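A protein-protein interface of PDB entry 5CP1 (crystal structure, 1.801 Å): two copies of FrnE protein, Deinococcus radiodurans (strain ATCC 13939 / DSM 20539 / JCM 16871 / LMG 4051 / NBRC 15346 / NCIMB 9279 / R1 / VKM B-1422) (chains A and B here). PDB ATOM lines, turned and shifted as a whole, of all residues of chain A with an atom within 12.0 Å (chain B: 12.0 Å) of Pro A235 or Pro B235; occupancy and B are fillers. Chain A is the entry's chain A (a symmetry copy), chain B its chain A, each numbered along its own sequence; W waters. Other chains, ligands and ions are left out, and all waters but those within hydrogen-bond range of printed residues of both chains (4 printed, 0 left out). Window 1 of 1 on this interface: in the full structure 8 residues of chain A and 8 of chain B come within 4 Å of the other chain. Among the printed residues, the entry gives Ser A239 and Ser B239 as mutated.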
ATOM      1  N   MET A 229     -25.103 -17.135   5.919  1.00  0.00           N
ATOM      2  CA  MET A 229     -24.362 -16.676   4.749  1.00  0.00           C
ATOM      3  C   MET A 229     -23.380 -17.715   4.233  1.00  0.00           C
ATOM      4  O   MET A 229     -22.621 -18.306   5.007  1.00  0.00           O
ATOM      5  CB  MET A 229     -23.621 -15.382   5.076  1.00  0.00           C
ATOM      6  CG  MET A 229     -24.554 -14.256   5.481  1.00  0.00           C
ATOM      7  SD  MET A 229     -25.765 -13.930   4.176  1.00  0.00           S
ATOM      8  CE  MET A 229     -24.662 -13.493   2.848  1.00  0.00           C
ATOM      9  N   LEU A 230     -23.396 -17.931   2.921  1.00  0.00           N
ATOM     10  CA  LEU A 230     -22.442 -18.819   2.267  1.00  0.00           C
ATOM     11  C   LEU A 230     -21.434 -18.011   1.478  1.00  0.00           C
ATOM     12  O   LEU A 230     -21.664 -16.841   1.182  1.00  0.00           O
ATOM     13  CB  LEU A 230     -23.140 -19.791   1.323  1.00  0.00           C
ATOM     14  CG  LEU A 230     -24.210 -20.716   1.883  1.00  0.00           C
ATOM     15  CD1 LEU A 230     -24.792 -21.523   0.743  1.00  0.00           C
ATOM     16  CD2 LEU A 230     -23.621 -21.629   2.938  1.00  0.00           C
ATOM     17  N   GLY A 231     -20.332 -18.651   1.113  1.00  0.00           N
ATOM     18  CA  GLY A 231     -19.301 -17.994   0.334  1.00  0.00           C
ATOM     19  C   GLY A 231     -18.708 -16.845   1.116  1.00  0.00           C
ATOM     20  O   GLY A 231     -18.565 -16.919   2.336  1.00  0.00           O
ATOM     21  N   GLN A 232     -18.380 -15.771   0.412  1.00  0.00           N
ATOM     22  CA  GLN A 232     -17.757 -14.617   1.043  1.00  0.00           C
ATOM     23  C   GLN A 232     -18.307 -13.336   0.422  1.00  0.00           C
ATOM     24  O   GLN A 232     -18.276 -13.177  -0.800  1.00  0.00           O
ATOM     25  CB  GLN A 232     -16.231 -14.706   0.909  1.00  0.00           C
ATOM     26  CG  GLN A 232     -15.440 -13.581   1.555  1.00  0.00           C
ATOM     27  CD  GLN A 232     -15.546 -13.529   3.079  1.00  0.00           C
ATOM     28  OE1 GLN A 232     -16.402 -14.164   3.688  1.00  0.00           O
ATOM     29  NE2 GLN A 232     -14.655 -12.763   3.699  1.00  0.00           N
ATOM     30  N   ASP A 233     -18.821 -12.443   1.269  1.00  0.00           N
ATOM     31  CA  ASP A 233     -19.519 -11.230   0.813  1.00  0.00           C
ATOM     32  C   ASP A 233     -18.718 -10.438  -0.207  1.00  0.00           C
ATOM     33  O   ASP A 233     -17.545 -10.148   0.011  1.00  0.00           O
ATOM     34  CB  ASP A 233     -19.858 -10.323   1.995  1.00  0.00           C
ATOM     35  CG  ASP A 233     -20.974 -10.874   2.842  1.00  0.00           C
ATOM     36  OD1 ASP A 233     -21.212 -12.101   2.793  1.00  0.00           O
ATOM     37  OD2 ASP A 233     -21.617 -10.077   3.554  1.00  0.00           O
ATOM     38  N   ALA A 234     -19.364 -10.093  -1.318  1.00  0.00           N
ATOM     39  CA  ALA A 234     -18.689  -9.430  -2.423  1.00  0.00           C
ATOM     40  C   ALA A 234     -18.248  -8.026  -2.026  1.00  0.00           C
ATOM     41  O   ALA A 234     -18.927  -7.355  -1.248  1.00  0.00           O
ATOM     42  CB  ALA A 234     -19.605  -9.378  -3.640  1.00  0.00           C
ATOM     43  N   PRO A 235     -17.096  -7.580  -2.553  1.00  0.00           N
ATOM     44  CA  PRO A 235     -16.665  -6.194  -2.329  1.00  0.00           C
ATOM     45  C   PRO A 235     -17.613  -5.213  -3.024  1.00  0.00           C
ATOM     46  O   PRO A 235     -18.169  -5.546  -4.067  1.00  0.00           O
ATOM     47  CB  PRO A 235     -15.263  -6.155  -2.946  1.00  0.00           C
ATOM     48  CG  PRO A 235     -15.266  -7.263  -3.969  1.00  0.00           C
ATOM     49  CD  PRO A 235     -16.137  -8.341  -3.374  1.00  0.00           C
ATOM     50  N   ALA A 236     -17.801  -4.021  -2.460  1.00  0.00           N
ATOM     51  CA  ALA A 236     -18.715  -3.057  -3.076  1.00  0.00           C
ATOM     52  C   ALA A 236     -17.994  -2.117  -4.035  1.00  0.00           C
ATOM     53  O   ALA A 236     -16.767  -2.073  -4.073  1.00  0.00           O
ATOM     54  CB  ALA A 236     -19.449  -2.254  -2.008  1.00  0.00           C
ATOM     55  N   GLU A 237     -18.768  -1.363  -4.811  1.00  0.00           N
ATOM     56  CA  GLU A 237     -18.201  -0.432  -5.782  1.00  0.00           C
ATOM     57  C   GLU A 237     -17.264   0.566  -5.096  1.00  0.00           C
ATOM     58  O   GLU A 237     -17.593   1.120  -4.050  1.00  0.00           O
ATOM     59  CB  GLU A 237     -19.317   0.297  -6.531  1.00  0.00           C
ATOM     60  CG  GLU A 237     -20.295  -0.628  -7.254  1.00  0.00           C
ATOM     61  CD  GLU A 237     -21.540   0.108  -7.741  1.00  0.00           C
ATOM     62  OE1 GLU A 237     -21.706   0.255  -8.972  1.00  0.00           O
ATOM     63  OE2 GLU A 237     -22.356   0.533  -6.889  1.00  0.00           O
ATOM     64  N   GLY A 238     -16.086   0.766  -5.682  1.00  0.00           N
ATOM     65  CA  GLY A 238     -15.070   1.623  -5.099  1.00  0.00           C
ATOM     66  C   GLY A 238     -13.927   0.827  -4.495  1.00  0.00           C
ATOM     67  O   GLY A 238     -12.921   1.393  -4.056  1.00  0.00           O
ATOM     68  N   SER A 239     -14.076  -0.493  -4.491  1.00  0.00           N
ATOM     69  CA  SER A 239     -13.104  -1.372  -3.853  1.00  0.00           C
ATOM     70  C   SER A 239     -12.296  -2.215  -4.839  1.00  0.00           C
ATOM     71  O   SER A 239     -12.396  -3.457  -4.856  1.00  0.00           O
ATOM     72  CB  SER A 239     -13.813  -2.282  -2.858  1.00  0.00           C
ATOM     73  OG  SER A 239     -14.453  -1.500  -1.867  1.00  0.00           O
ATOM     74  N   GLU A 240     -11.485  -1.528  -5.643  1.00  0.00           N
ATOM     75  CA  GLU A 240     -10.511  -2.173  -6.531  1.00  0.00           C
ATOM     76  C   GLU A 240      -9.311  -2.703  -5.762  1.00  0.00           C
ATOM     77  O   GLU A 240      -8.173  -2.268  -5.979  1.00  0.00           O
ATOM     78  CB  GLU A 240     -10.038  -1.194  -7.600  1.00  0.00           C
ATOM     79  CG  GLU A 240     -11.044  -1.019  -8.693  1.00  0.00           C
ATOM     80  CD  GLU A 240     -11.491  -2.356  -9.233  1.00  0.00           C
ATOM     81  OE1 GLU A 240     -10.694  -2.998  -9.945  1.00  0.00           O
ATOM     82  OE2 GLU A 240     -12.630  -2.776  -8.927  1.00  0.00           O
ATOM     83  N   ASP A 241      -9.573  -3.647  -4.866  1.00  0.00           N
ATOM     84  CA  ASP A 241      -8.581  -4.065  -3.891  1.00  0.00           C
ATOM     85  C   ASP A 241      -8.468  -5.563  -3.908  1.00  0.00           C
ATOM     86  O   ASP A 241      -9.293  -6.262  -4.509  1.00  0.00           O
ATOM     87  CB  ASP A 241      -8.948  -3.629  -2.466  1.00  0.00           C
ATOM     88  CG  ASP A 241      -9.444  -2.214  -2.388  1.00  0.00           C
ATOM     89  OD1 ASP A 241      -8.969  -1.362  -3.169  1.00  0.00           O
ATOM     90  OD2 ASP A 241     -10.314  -1.957  -1.528  1.00  0.00           O
ATOM     91  N   GLY A 242      -7.468  -6.060  -3.200  1.00  0.00           N
ATOM     92  CA  GLY A 242      -7.327  -7.491  -3.051  1.00  0.00           C
ATOM     93  C   GLY A 242      -6.258  -7.792  -2.034  1.00  0.00           C
ATOM     94  O   GLY A 242      -5.466  -6.925  -1.651  1.00  0.00           O
ATOM     95  N   GLN A 243      -6.251  -9.036  -1.584  1.00  0.00           N
ATOM     96  CA  GLN A 243      -5.159  -9.539  -0.779  1.00  0.00           C
ATOM     97  C   GLN A 243      -4.917 -10.966  -1.206  1.00  0.00           C
ATOM     98  O   GLN A 243      -5.758 -11.569  -1.874  1.00  0.00           O
ATOM     99  CB  GLN A 243      -5.490  -9.471   0.706  1.00  0.00           C
ATOM    100  CG  GLN A 243      -6.724 -10.283   1.073  1.00  0.00           C
ATOM    101  CD  GLN A 243      -7.048 -10.214   2.546  1.00  0.00           C
ATOM    102  OE1 GLN A 243      -8.074  -9.660   2.945  1.00  0.00           O
ATOM    103  NE2 GLN A 243      -6.175 -10.775   3.366  1.00  0.00           N
ATOM    104  N   CYS A 244      -3.757 -11.490  -0.845  1.00  0.00           N
ATOM    105  CA  CYS A 244      -3.511 -12.919  -0.933  1.00  0.00           C
ATOM    106  C   CYS A 244      -3.645 -13.483   0.462  1.00  0.00           C
ATOM    107  O   CYS A 244      -2.975 -13.012   1.380  1.00  0.00           O
ATOM    108  CB  CYS A 244      -2.119 -13.224  -1.488  1.00  0.00           C
ATOM    109  SG  CYS A 244      -1.714 -12.337  -2.988  1.00  0.00           S
ATOM    110  N   ALA A 245      -4.508 -14.481   0.616  1.00  0.00           N
ATOM    111  CA  ALA A 245      -4.753 -15.100   1.915  1.00  0.00           C
ATOM    112  C   ALA A 245      -3.965 -16.395   2.056  1.00  0.00           C
ATOM    113  O   ALA A 245      -3.567 -17.009   1.060  1.00  0.00           O
ATOM    114  CB  ALA A 245      -6.246 -15.362   2.106  1.00  0.00           C
ATOM    115  N   VAL A 246      -3.723 -16.804   3.295  1.00  0.00           N
ATOM    116  CA  VAL A 246      -3.014 -18.049   3.547  1.00  0.00           C
ATOM    117  C   VAL A 246      -3.919 -19.224   3.195  1.00  0.00           C
ATOM    118  O   VAL A 246      -5.138 -19.092   3.257  1.00  0.00           O
ATOM    119  CB  VAL A 246      -2.561 -18.160   5.014  1.00  0.00           C
ATOM    120  CG1 VAL A 246      -1.543 -17.085   5.330  1.00  0.00           C
ATOM    121  CG2 VAL A 246      -3.759 -18.068   5.948  1.00  0.00           C
ATOM    122  N   GLN A 248      -6.266 -22.141   3.396  1.00  0.00           N
ATOM    123  CA  GLN A 248      -7.249 -22.454   4.424  1.00  0.00           C
ATOM    124  C   GLN A 248      -8.195 -23.565   3.974  1.00  0.00           C
ATOM    125  O   GLN A 248      -7.766 -24.683   3.684  1.00  0.00           O
ATOM    126  CB  GLN A 248      -8.042 -21.201   4.787  1.00  0.00           C
ATOM    127  CG  GLN A 248      -8.780 -20.594   3.606  1.00  0.00           C
ATOM    128  CD  GLN A 248      -9.540 -19.338   3.976  1.00  0.00           C
ATOM    129  OE1 GLN A 248      -8.952 -18.358   4.437  1.00  0.00           O
ATOM    130  NE2 GLN A 248     -10.856 -19.360   3.780  1.00  0.00           N
ATOM    131  N   MET B 229      -9.970  -2.480  13.077  1.00  0.00           N
ATOM    132  CA  MET B 229      -9.895  -2.498  11.620  1.00  0.00           C
ATOM    133  C   MET B 229     -10.519  -1.266  10.985  1.00  0.00           C
ATOM    134  O   MET B 229     -11.631  -0.865  11.345  1.00  0.00           O
ATOM    135  CB  MET B 229     -10.569  -3.756  11.080  1.00  0.00           C
ATOM    136  CG  MET B 229      -9.916  -5.033  11.574  1.00  0.00           C
ATOM    137  SD  MET B 229      -8.162  -5.067  11.131  1.00  0.00           S
ATOM    138  CE  MET B 229      -8.301  -4.984   9.357  1.00  0.00           C
ATOM    139  N   LEU B 230      -9.801  -0.672  10.037  1.00  0.00           N
ATOM    140  CA  LEU B 230     -10.312   0.455   9.265  1.00  0.00           C
ATOM    141  C   LEU B 230     -10.636   0.016   7.854  1.00  0.00           C
ATOM    142  O   LEU B 230     -10.174  -1.028   7.402  1.00  0.00           O
ATOM    143  CB  LEU B 230      -9.302   1.596   9.206  1.00  0.00           C
ATOM    144  CG  LEU B 230      -8.811   2.208  10.509  1.00  0.00           C
ATOM    145  CD1 LEU B 230      -7.773   3.261  10.183  1.00  0.00           C
ATOM    146  CD2 LEU B 230      -9.967   2.816  11.276  1.00  0.00           C
ATOM    147  N   GLY B 231     -11.407   0.835   7.151  1.00  0.00           N
ATOM    148  CA  GLY B 231     -11.769   0.538   5.779  1.00  0.00           C
ATOM    149  C   GLY B 231     -12.586  -0.731   5.718  1.00  0.00           C
ATOM    150  O   GLY B 231     -13.385  -1.012   6.610  1.00  0.00           O
ATOM    151  N   GLN B 232     -12.369  -1.512   4.669  1.00  0.00           N
ATOM    152  CA  GLN B 232     -13.127  -2.739   4.472  1.00  0.00           C
ATOM    153  C   GLN B 232     -12.210  -3.821   3.911  1.00  0.00           C
ATOM    154  O   GLN B 232     -11.545  -3.605   2.895  1.00  0.00           O
ATOM    155  CB  GLN B 232     -14.325  -2.473   3.551  1.00  0.00           C
ATOM    156  CG  GLN B 232     -15.234  -3.661   3.281  1.00  0.00           C
ATOM    157  CD  GLN B 232     -15.983  -4.175   4.511  1.00  0.00           C
ATOM    158  OE1 GLN B 232     -15.669  -3.831   5.647  1.00  0.00           O
ATOM    159  NE2 GLN B 232     -16.992  -5.004   4.272  1.00  0.00           N
ATOM    160  N   ASP B 233     -12.169  -4.969   4.588  1.00  0.00           N
ATOM    161  CA  ASP B 233     -11.227  -6.051   4.257  1.00  0.00           C
ATOM    162  C   ASP B 233     -11.254  -6.426   2.784  1.00  0.00           C
ATOM    163  O   ASP B 233     -12.319  -6.658   2.219  1.00  0.00           O
ATOM    164  CB  ASP B 233     -11.515  -7.296   5.095  1.00  0.00           C
ATOM    165  CG  ASP B 233     -11.110  -7.129   6.534  1.00  0.00           C
ATOM    166  OD1 ASP B 233     -10.999  -5.971   6.994  1.00  0.00           O
ATOM    167  OD2 ASP B 233     -10.897  -8.158   7.206  1.00  0.00           O
ATOM    168  N   ALA B 234     -10.073  -6.482   2.174  1.00  0.00           N
ATOM    169  CA  ALA B 234      -9.960  -6.720   0.743  1.00  0.00           C
ATOM    170  C   ALA B 234     -10.415  -8.131   0.390  1.00  0.00           C
ATOM    171  O   ALA B 234     -10.220  -9.064   1.171  1.00  0.00           O
ATOM    172  CB  ALA B 234      -8.524  -6.491   0.286  1.00  0.00           C
ATOM    173  N   PRO B 235     -11.036  -8.292  -0.789  1.00  0.00           N
ATOM    174  CA  PRO B 235     -11.389  -9.635  -1.266  1.00  0.00           C
ATOM    175  C   PRO B 235     -10.129 -10.448  -1.575  1.00  0.00           C
ATOM    176  O   PRO B 235      -9.123  -9.872  -1.981  1.00  0.00           O
ATOM    177  CB  PRO B 235     -12.206  -9.359  -2.533  1.00  0.00           C
ATOM    178  CG  PRO B 235     -11.740  -8.001  -2.997  1.00  0.00           C
ATOM    179  CD  PRO B 235     -11.447  -7.235  -1.732  1.00  0.00           C
ATOM    180  N   ALA B 236     -10.174 -11.766  -1.388  1.00  0.00           N
ATOM    181  CA  ALA B 236      -8.988 -12.583  -1.649  1.00  0.00           C
ATOM    182  C   ALA B 236      -8.968 -13.123  -3.074  1.00  0.00           C
ATOM    183  O   ALA B 236      -9.959 -13.040  -3.795  1.00  0.00           O
ATOM    184  CB  ALA B 236      -8.895 -13.732  -0.652  1.00  0.00           C
ATOM    185  N   GLU B 237      -7.828 -13.680  -3.475  1.00  0.00           N
ATOM    186  CA  GLU B 237      -7.675 -14.223  -4.822  1.00  0.00           C
ATOM    187  C   GLU B 237      -8.738 -15.289  -5.103  1.00  0.00           C
ATOM    188  O   GLU B 237      -8.992 -16.158  -4.272  1.00  0.00           O
ATOM    189  CB  GLU B 237      -6.269 -14.796  -5.006  1.00  0.00           C
ATOM    190  CG  GLU B 237      -5.145 -13.792  -4.753  1.00  0.00           C
ATOM    191  CD  GLU B 237      -3.777 -14.461  -4.662  1.00  0.00           C
ATOM    192  OE1 GLU B 237      -2.946 -14.249  -5.573  1.00  0.00           O
ATOM    193  OE2 GLU B 237      -3.533 -15.194  -3.675  1.00  0.00           O
ATOM    194  N   GLY B 238      -9.371 -15.195  -6.270  1.00  0.00           N
ATOM    195  CA  GLY B 238     -10.456 -16.089  -6.633  1.00  0.00           C
ATOM    196  C   GLY B 238     -11.809 -15.407  -6.557  1.00  0.00           C
ATOM    197  O   GLY B 238     -12.833 -15.982  -6.940  1.00  0.00           O
ATOM    198  N   SER B 239     -11.811 -14.167  -6.078  1.00  0.00           N
ATOM    199  CA  SER B 239     -13.050 -13.433  -5.857  1.00  0.00           C
ATOM    200  C   SER B 239     -13.252 -12.263  -6.820  1.00  0.00           C
ATOM    201  O   SER B 239     -13.275 -11.088  -6.408  1.00  0.00           O
ATOM    202  CB  SER B 239     -13.097 -12.930  -4.419  1.00  0.00           C
ATOM    203  OG  SER B 239     -13.041 -14.027  -3.527  1.00  0.00           O
ATOM    204  N   GLU B 240     -13.416 -12.601  -8.099  1.00  0.00           N
ATOM    205  CA  GLU B 240     -13.792 -11.633  -9.136  1.00  0.00           C
ATOM    206  C   GLU B 240     -15.260 -11.248  -9.042  1.00  0.00           C
ATOM    207  O   GLU B 240     -16.043 -11.491  -9.970  1.00  0.00           O
ATOM    208  CB  GLU B 240     -13.502 -12.201 -10.521  1.00  0.00           C
ATOM    209  CG  GLU B 240     -12.050 -12.135 -10.867  1.00  0.00           C
ATOM    210  CD  GLU B 240     -11.504 -10.746 -10.642  1.00  0.00           C
ATOM    211  OE1 GLU B 240     -11.830  -9.850 -11.446  1.00  0.00           O
ATOM    212  OE2 GLU B 240     -10.769 -10.542  -9.650  1.00  0.00           O
ATOM    213  N   ASP B 241     -15.625 -10.642  -7.919  1.00  0.00           N
ATOM    214  CA  ASP B 241     -17.025 -10.444  -7.584  1.00  0.00           C
ATOM    215  C   ASP B 241     -17.248  -9.005  -7.213  1.00  0.00           C
ATOM    216  O   ASP B 241     -16.296  -8.239  -7.017  1.00  0.00           O
ATOM    217  CB  ASP B 241     -17.468 -11.317  -6.401  1.00  0.00           C
ATOM    218  CG  ASP B 241     -16.968 -12.731  -6.488  1.00  0.00           C
ATOM    219  OD1 ASP B 241     -16.852 -13.263  -7.612  1.00  0.00           O
ATOM    220  OD2 ASP B 241     -16.700 -13.311  -5.415  1.00  0.00           O
ATOM    221  N   GLY B 242     -18.513  -8.651  -7.066  1.00  0.00           N
ATOM    222  CA  GLY B 242     -18.844  -7.324  -6.602  1.00  0.00           C
ATOM    223  C   GLY B 242     -20.320  -7.241  -6.311  1.00  0.00           C
ATOM    224  O   GLY B 242     -21.107  -8.106  -6.709  1.00  0.00           O
ATOM    225  N   GLN B 243     -20.690  -6.193  -5.594  1.00  0.00           N
ATOM    226  CA  GLN B 243     -22.086  -5.854  -5.421  1.00  0.00           C
ATOM    227  C   GLN B 243     -22.182  -4.349  -5.462  1.00  0.00           C
ATOM    228  O   GLN B 243     -21.172  -3.654  -5.337  1.00  0.00           O
ATOM    229  CB  GLN B 243     -22.626  -6.391  -4.102  1.00  0.00           C
ATOM    230  CG  GLN B 243     -21.882  -5.844  -2.892  1.00  0.00           C
ATOM    231  CD  GLN B 243     -22.420  -6.378  -1.588  1.00  0.00           C
ATOM    232  OE1 GLN B 243     -21.740  -7.118  -0.875  1.00  0.00           O
ATOM    233  NE2 GLN B 243     -23.649  -6.009  -1.265  1.00  0.00           N
ATOM    234  N   CYS B 244     -23.390  -3.850  -5.666  1.00  0.00           N
ATOM    235  CA  CYS B 244     -23.678  -2.444  -5.444  1.00  0.00           C
ATOM    236  C   CYS B 244     -24.391  -2.337  -4.116  1.00  0.00           C
ATOM    237  O   CYS B 244     -25.409  -2.996  -3.912  1.00  0.00           O
ATOM    238  CB  CYS B 244     -24.553  -1.860  -6.555  1.00  0.00           C
ATOM    239  SG  CYS B 244     -23.978  -2.218  -8.210  1.00  0.00           S
ATOM    240  N   ALA B 245     -23.853  -1.514  -3.222  1.00  0.00           N
ATOM    241  CA  ALA B 245     -24.425  -1.335  -1.891  1.00  0.00           C
ATOM    242  C   ALA B 245     -25.276  -0.074  -1.831  1.00  0.00           C
ATOM    243  O   ALA B 245     -25.111   0.843  -2.643  1.00  0.00           O
ATOM    244  CB  ALA B 245     -23.318  -1.282  -0.839  1.00  0.00           C
ATOM    245  N   VAL B 246     -26.199  -0.032  -0.878  1.00  0.00           N
ATOM    246  CA  VAL B 246     -27.040   1.141  -0.704  1.00  0.00           C
ATOM    247  C   VAL B 246     -26.205   2.278  -0.127  1.00  0.00           C
ATOM    248  O   VAL B 246     -25.217   2.022   0.556  1.00  0.00           O
ATOM    249  CB  VAL B 246     -28.236   0.851   0.222  1.00  0.00           C
ATOM    250  CG1 VAL B 246     -29.155  -0.170  -0.416  1.00  0.00           C
ATOM    251  CG2 VAL B 246     -27.752   0.374   1.583  1.00  0.00           C
ATOM    252  N   GLN B 248     -24.642   4.772   2.195  1.00  0.00           N
ATOM    253  CA  GLN B 248     -24.425   4.673   3.632  1.00  0.00           C
ATOM    254  C   GLN B 248     -23.496   5.775   4.136  1.00  0.00           C
ATOM    255  O   GLN B 248     -23.794   6.963   4.006  1.00  0.00           O
ATOM    256  CB  GLN B 248     -23.852   3.301   3.980  1.00  0.00           C
ATOM    257  CG  GLN B 248     -22.533   3.007   3.288  1.00  0.00           C
ATOM    258  CD  GLN B 248     -21.992   1.633   3.621  1.00  0.00           C
ATOM    259  OE1 GLN B 248     -22.642   0.619   3.363  1.00  0.00           O
ATOM    260  NE2 GLN B 248     -20.795   1.591   4.202  1.00  0.00           N
HETATM  261  O   HOH W   1      -8.983 -10.832   6.024  1.00  0.00           O
HETATM  262  O   HOH W   2     -16.893 -12.330  -2.911  1.00  0.00           O
HETATM  263  O   HOH W   3     -11.447  -3.653   0.235  1.00  0.00           O
HETATM  264  O   HOH W   4     -22.797  -7.007   2.373  1.00  0.00           O
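Ala A234 touches Asp B241 (CB to CB, 3.99 Å).
Ala A234 touches Gly B242 (CB to C, 3.5 Å).
CG of Pro A235 touches CG of Pro B235, 3.7 Å away.
CA of Gly B242 touches O of Pro A235, at 3.2 Å.
Gln B243 touches Ala A236.
Asp A241 touches Ala B234.
O of Asp A241 touches CG of Pro B235, at 3.4 Å.
C of Gly A242 touches CB of Ala B234, at 3.5 Å.
Pro B235 touches Gly A242 (O to CA, 3.2 Å).
CA of Ala B236 touches O of Gln A243 (3.4 Å).
O of Ala B236 lies close to OG of Ser B239.
O of Ala A236 lies close to OG of Ser A239 (3.2 Å).
The backbone carbonyl oxygen of Ala B234 lies close to the side-chain amide oxygen of Gln A243, at 2.8 Å.
The backbone carbonyl oxygen (O) of Pro B235 lies within hydrogen-bond range of the backbone NH (N) of Gln A243, at 3.0 Å.
The backbone NH (N) of Glu B237 lies within hydrogen-bond range of the backbone carbonyl oxygen (O) of Gln A243 (3.4 Å).
The side-chain carboxylate of Glu B237 sits close to the side-chain sulfur of Cys A244, at 3.4 Å.
O of Ala A234 sits close to OE1 of Gln B243 (2.8 Å).
The backbone NH of Gln B243 is in hydrogen-bond range of the backbone carbonyl oxygen of Pro A235 (3.0 Å).
The backbone carbonyl oxygen of Gln B243 lies within hydrogen-bond range of the backbone NH of Glu A237, 3.4 Å away.
OE1 of Glu A237 sits close to SG of Cys B244.
Ala A234 touches Asp B241, and with the chains exchanged Asp A241 touches Ala B234.
Pro A235 touches Asp B241, and with the chains exchanged Asp A241 touches Pro B235.
Pro A235 touches Gly B242, and with the chains exchanged Gly A242 touches Pro B235.
Ala A236 touches Gln B243, and with the chains exchanged Gln A243 touches Ala B236.
Water W3 lies within hydrogen-bond range of the backbone carbonyl oxygen (O) of Gln B232 (2.7 Å) and the side-chain carboxylate (OD2) of Asp A241 (2.7 Å).
Water W2 lies within hydrogen-bond range of the backbone carbonyl oxygen (O) of Gln A232 and the side-chain carboxylate (OD2) of Asp B241.
Water W4 bridges OE1 of Gln B243 (3.4 Å) and OD2 of Asp A233 (3.5 Å).
Water W1 lies within hydrogen-bond range of the side-chain amide oxygen (OE1) of Gln A243 (3.4 Å) and the side-chain carboxylate (OD2) of Asp B233 (3.5 Å).
Of the 19 printed residues of chain B, 8 touch a printed residue of chain A.
Hydrophobic or aromatic side chains of chain B that line the printed part of chain A: Ala B234 and Pro B235.
Met A229 touches none of the printed residues of chain B.
Of the printed residues of chain B, Ala A234 touches Asp B241, Gly B242 and Gln B243.
Of chain B, only Pro B235, Asp B241, Gly B242 and Gln B243 come within 4 Å of Pro A235.
Of the printed residues of chain B, Ala A236 touches Gln B243.
Gly A242 touches just these residues of chain B: Ala B234 and Pro B235.
Gln A243 touches just these residues of chain B: Ala B234 (2.8 Å), Pro B235 (3.0 Å), Ala B236 (3.4 Å) and Glu B237 (3.4 Å).
Cys A244 touches one residue of chain B.
Of chain A, only Pro A235, Asp A241, Gly A242 and Gln A243 come within 4 Å of Pro B235.
Ala B236 touches just one residue of chain A: Gln A243 (3.4 Å).
No residue of chain A comes within 4 Å of Ser B239.
Of the printed residues of chain A, Asp B241 touches Ala A234 (3.99 Å) and Pro A235 (3.4 Å).
Of chain A, only Ala A234 and Pro A235 come within 4 Å of Gly B242.
Gln B243 touches just these residues of chain A: Ala A234, Pro A235, Ala A236 and Glu A237.
Cys B244 touches just one residue of chain A: Glu A237.
Val B246 touches none of the printed residues of chain A.
The nearest residue of chain A that does not touch Pro B235 is Ser A239 (5.0 Å).
The nearest printed residue of chain A that does not touch Ala B234 is Pro A235 (6.2 Å).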
